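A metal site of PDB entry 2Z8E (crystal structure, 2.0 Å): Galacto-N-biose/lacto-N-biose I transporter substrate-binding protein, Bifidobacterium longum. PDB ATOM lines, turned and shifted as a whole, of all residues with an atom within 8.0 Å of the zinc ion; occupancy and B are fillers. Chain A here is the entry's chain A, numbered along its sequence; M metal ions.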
ATOM      1  N   ASP A  11     -18.490  10.762  31.826  1.00  0.00           N
ATOM      2  CA  ASP A  11     -18.879   9.749  30.794  1.00  0.00           C
ATOM      3  C   ASP A  11     -19.194  10.415  29.456  1.00  0.00           C
ATOM      4  O   ASP A  11     -19.675  11.568  29.396  1.00  0.00           O
ATOM      5  CB  ASP A  11     -20.100   8.932  31.268  1.00  0.00           C
ATOM      6  CG  ASP A  11     -19.725   7.607  31.895  1.00  0.00           C
ATOM      7  OD1 ASP A  11     -18.510   7.284  32.055  1.00  0.00           O
ATOM      8  OD2 ASP A  11     -20.674   6.863  32.245  1.00  0.00           O
ATOM      9  N   ASP A  12     -18.919   9.722  28.359  1.00  0.00           N
ATOM     10  CA  ASP A  12     -19.384  10.171  27.042  1.00  0.00           C
ATOM     11  C   ASP A  12     -20.877  10.404  27.039  1.00  0.00           C
ATOM     12  O   ASP A  12     -21.580   9.889  27.905  1.00  0.00           O
ATOM     13  CB  ASP A  12     -19.086   9.098  25.981  1.00  0.00           C
ATOM     14  CG  ASP A  12     -17.628   8.804  25.834  1.00  0.00           C
ATOM     15  OD1 ASP A  12     -16.793   9.655  26.197  1.00  0.00           O
ATOM     16  OD2 ASP A  12     -17.328   7.697  25.336  1.00  0.00           O
ATOM     17  N   GLY A  13     -21.376  11.105  26.035  1.00  0.00           N
ATOM     18  CA  GLY A  13     -22.802  11.207  25.798  1.00  0.00           C
ATOM     19  C   GLY A  13     -23.337   9.896  25.242  1.00  0.00           C
ATOM     20  O   GLY A  13     -22.568   8.957  24.985  1.00  0.00           O
ATOM     21  N   VAL A  16     -21.758   7.626  20.795  1.00  0.00           N
ATOM     22  CA  VAL A  16     -20.432   7.928  20.311  1.00  0.00           C
ATOM     23  C   VAL A  16     -20.300   7.486  18.849  1.00  0.00           C
ATOM     24  O   VAL A  16     -20.766   6.419  18.492  1.00  0.00           O
ATOM     25  CB  VAL A  16     -19.378   7.263  21.228  1.00  0.00           C
ATOM     26  CG1 VAL A  16     -18.075   6.948  20.463  1.00  0.00           C
ATOM     27  CG2 VAL A  16     -19.095   8.174  22.424  1.00  0.00           C
ATOM     28  N   ASN A  17     -19.690   8.324  18.011  1.00  0.00           N
ATOM     29  CA  ASN A  17     -19.505   8.017  16.589  1.00  0.00           C
ATOM     30  C   ASN A  17     -18.035   7.757  16.283  1.00  0.00           C
ATOM     31  O   ASN A  17     -17.168   8.566  16.619  1.00  0.00           O
ATOM     32  CB  ASN A  17     -20.061   9.130  15.697  1.00  0.00           C
ATOM     33  CG  ASN A  17     -21.597   9.234  15.732  1.00  0.00           C
ATOM     34  OD1 ASN A  17     -22.310   8.381  15.209  1.00  0.00           O
ATOM     35  ND2 ASN A  17     -22.098  10.325  16.331  1.00  0.00           N
ATOM     36  N   ILE A  18     -17.778   6.610  15.668  1.00  0.00           N
ATOM     37  CA  ILE A  18     -16.426   6.118  15.385  1.00  0.00           C
ATOM     38  C   ILE A  18     -16.272   5.951  13.866  1.00  0.00           C
ATOM     39  O   ILE A  18     -17.162   5.483  13.182  1.00  0.00           O
ATOM     40  CB  ILE A  18     -16.195   4.758  16.108  1.00  0.00           C
ATOM     41  CG1 ILE A  18     -16.251   4.934  17.623  1.00  0.00           C
ATOM     42  CG2 ILE A  18     -14.859   4.073  15.691  1.00  0.00           C
ATOM     43  CD1 ILE A  18     -15.198   5.891  18.177  1.00  0.00           C
ATOM     44  N   ASP A  46     -25.096   2.975  21.126  1.00  0.00           N
ATOM     45  CA  ASP A  46     -24.194   3.811  21.941  1.00  0.00           C
ATOM     46  C   ASP A  46     -22.789   4.055  21.336  1.00  0.00           C
ATOM     47  O   ASP A  46     -22.064   4.972  21.770  1.00  0.00           O
ATOM     48  CB  ASP A  46     -24.038   3.207  23.363  1.00  0.00           C
ATOM     49  CG  ASP A  46     -23.497   1.768  23.356  1.00  0.00           C
ATOM     50  OD1 ASP A  46     -24.049   0.874  22.659  1.00  0.00           O
ATOM     51  OD2 ASP A  46     -22.544   1.503  24.087  1.00  0.00           O
ATOM     52  N   ILE A  47     -22.394   3.204  20.386  1.00  0.00           N
ATOM     53  CA  ILE A  47     -21.134   3.350  19.630  1.00  0.00           C
ATOM     54  C   ILE A  47     -21.410   3.017  18.151  1.00  0.00           C
ATOM     55  O   ILE A  47     -21.463   1.853  17.772  1.00  0.00           O
ATOM     56  CB  ILE A  47     -20.004   2.415  20.130  1.00  0.00           C
ATOM     57  CG1 ILE A  47     -19.736   2.614  21.627  1.00  0.00           C
ATOM     58  CG2 ILE A  47     -18.687   2.668  19.273  1.00  0.00           C
ATOM     59  CD1 ILE A  47     -19.036   1.395  22.310  1.00  0.00           C
ATOM     60  N   TYR A 100      -6.120   0.037  27.060  1.00  0.00           N
ATOM     61  CA  TYR A 100      -7.278  -0.579  26.421  1.00  0.00           C
ATOM     62  C   TYR A 100      -6.907  -1.903  25.733  1.00  0.00           C
ATOM     63  O   TYR A 100      -7.595  -2.911  25.921  1.00  0.00           O
ATOM     64  CB  TYR A 100      -7.882   0.400  25.420  1.00  0.00           C
ATOM     65  CG  TYR A 100      -8.242   1.733  26.015  1.00  0.00           C
ATOM     66  CD1 TYR A 100      -9.109   1.831  27.100  1.00  0.00           C
ATOM     67  CD2 TYR A 100      -7.732   2.903  25.477  1.00  0.00           C
ATOM     68  CE1 TYR A 100      -9.447   3.058  27.645  1.00  0.00           C
ATOM     69  CE2 TYR A 100      -8.057   4.135  26.005  1.00  0.00           C
ATOM     70  CZ  TYR A 100      -8.927   4.203  27.091  1.00  0.00           C
ATOM     71  OH  TYR A 100      -9.219   5.446  27.596  1.00  0.00           O
ATOM     72  N   SER A 298      -7.885  10.772  17.944  1.00  0.00           N
ATOM     73  CA  SER A 298      -9.172  10.151  18.281  1.00  0.00           C
ATOM     74  C   SER A 298      -9.588  10.569  19.694  1.00  0.00           C
ATOM     75  O   SER A 298      -8.812  10.453  20.620  1.00  0.00           O
ATOM     76  CB  SER A 298      -9.101   8.627  18.219  1.00  0.00           C
ATOM     77  OG  SER A 298     -10.388   8.058  18.518  1.00  0.00           O
ATOM     78  N   LYS A 299     -10.802  11.058  19.834  1.00  0.00           N
ATOM     79  CA  LYS A 299     -11.365  11.417  21.157  1.00  0.00           C
ATOM     80  C   LYS A 299     -11.967  10.238  21.880  1.00  0.00           C
ATOM     81  O   LYS A 299     -12.246  10.335  23.110  1.00  0.00           O
ATOM     82  CB  LYS A 299     -12.398  12.544  21.062  1.00  0.00           C
ATOM     83  CG  LYS A 299     -11.877  13.861  20.410  1.00  0.00           C
ATOM     84  CD  LYS A 299     -10.659  14.489  21.153  1.00  0.00           C
ATOM     85  CE  LYS A 299     -11.052  15.575  22.210  1.00  0.00           C
ATOM     86  NZ  LYS A 299     -11.824  16.782  21.676  1.00  0.00           N
ATOM     87  N   HIS A 300     -12.158   9.130  21.160  1.00  0.00           N
ATOM     88  CA  HIS A 300     -12.794   7.942  21.736  1.00  0.00           C
ATOM     89  C   HIS A 300     -12.019   6.621  21.627  1.00  0.00           C
ATOM     90  O   HIS A 300     -12.572   5.605  21.160  1.00  0.00           O
ATOM     91  CB  HIS A 300     -14.212   7.787  21.206  1.00  0.00           C
ATOM     92  CG  HIS A 300     -15.089   8.940  21.584  1.00  0.00           C
ATOM     93  ND1 HIS A 300     -15.612   9.083  22.853  1.00  0.00           N
ATOM     94  CD2 HIS A 300     -15.493  10.022  20.884  1.00  0.00           C
ATOM     95  CE1 HIS A 300     -16.327  10.202  22.911  1.00  0.00           C
ATOM     96  NE2 HIS A 300     -16.274  10.789  21.728  1.00  0.00           N
ATOM     97  N   PRO A 301     -10.765   6.628  22.138  1.00  0.00           N
ATOM     98  CA  PRO A 301      -9.914   5.430  22.124  1.00  0.00           C
ATOM     99  C   PRO A 301     -10.587   4.201  22.724  1.00  0.00           C
ATOM    100  O   PRO A 301     -10.469   3.112  22.156  1.00  0.00           O
ATOM    101  CB  PRO A 301      -8.694   5.840  22.939  1.00  0.00           C
ATOM    102  CG  PRO A 301      -9.094   7.175  23.643  1.00  0.00           C
ATOM    103  CD  PRO A 301     -10.066   7.794  22.719  1.00  0.00           C
ATOM    104  N   LYS A 302     -11.298   4.392  23.853  1.00  0.00           N
ATOM    105  CA  LYS A 302     -11.841   3.258  24.563  1.00  0.00           C
ATOM    106  C   LYS A 302     -12.870   2.557  23.720  1.00  0.00           C
ATOM    107  O   LYS A 302     -12.850   1.329  23.632  1.00  0.00           O
ATOM    108  CB  LYS A 302     -12.468   3.627  25.914  1.00  0.00           C
ATOM    109  CG  LYS A 302     -12.896   2.340  26.655  1.00  0.00           C
ATOM    110  CD  LYS A 302     -13.211   2.535  28.123  1.00  0.00           C
ATOM    111  CE  LYS A 302     -13.751   1.228  28.666  1.00  0.00           C
ATOM    112  NZ  LYS A 302     -13.795   1.123  30.177  1.00  0.00           N
ATOM    113  N   GLU A 303     -13.775   3.326  23.102  1.00  0.00           N
ATOM    114  CA  GLU A 303     -14.860   2.706  22.318  1.00  0.00           C
ATOM    115  C   GLU A 303     -14.383   2.267  20.956  1.00  0.00           C
ATOM    116  O   GLU A 303     -14.856   1.285  20.433  1.00  0.00           O
ATOM    117  CB  GLU A 303     -16.083   3.640  22.163  1.00  0.00           C
ATOM    118  CG  GLU A 303     -16.759   3.996  23.496  1.00  0.00           C
ATOM    119  CD  GLU A 303     -15.989   5.023  24.300  1.00  0.00           C
ATOM    120  OE1 GLU A 303     -15.639   6.074  23.743  1.00  0.00           O
ATOM    121  OE2 GLU A 303     -15.720   4.801  25.509  1.00  0.00           O
ATOM    122  N   ALA A 304     -13.419   2.983  20.383  1.00  0.00           N
ATOM    123  CA  ALA A 304     -12.787   2.538  19.148  1.00  0.00           C
ATOM    124  C   ALA A 304     -12.202   1.137  19.316  1.00  0.00           C
ATOM    125  O   ALA A 304     -12.342   0.260  18.430  1.00  0.00           O
ATOM    126  CB  ALA A 304     -11.710   3.534  18.714  1.00  0.00           C
HETATM  127 ZN    ZN M   1     -15.397   7.834  24.431  1.00  0.00          ZN
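The zinc ion is bound by the side-chain carboxylate of Glu 303 (1.9 Å), a ring nitrogen (ND1) of His 300 (2.0 Å) and the side-chain carboxylate of Asp 12 (2.1 Å). The zinc ion has three donor atoms within binding distance.
Three residues have an atom within 4 Å of the zinc ion: Asp 12, His 300 and Glu 303. The nearest printed residue that does not touch the zinc ion is Val 16 (4.2 Å).
The backbone NH of His 300 sits close to the side-chain hydroxyl of Ser 298, at 3.4 Å.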
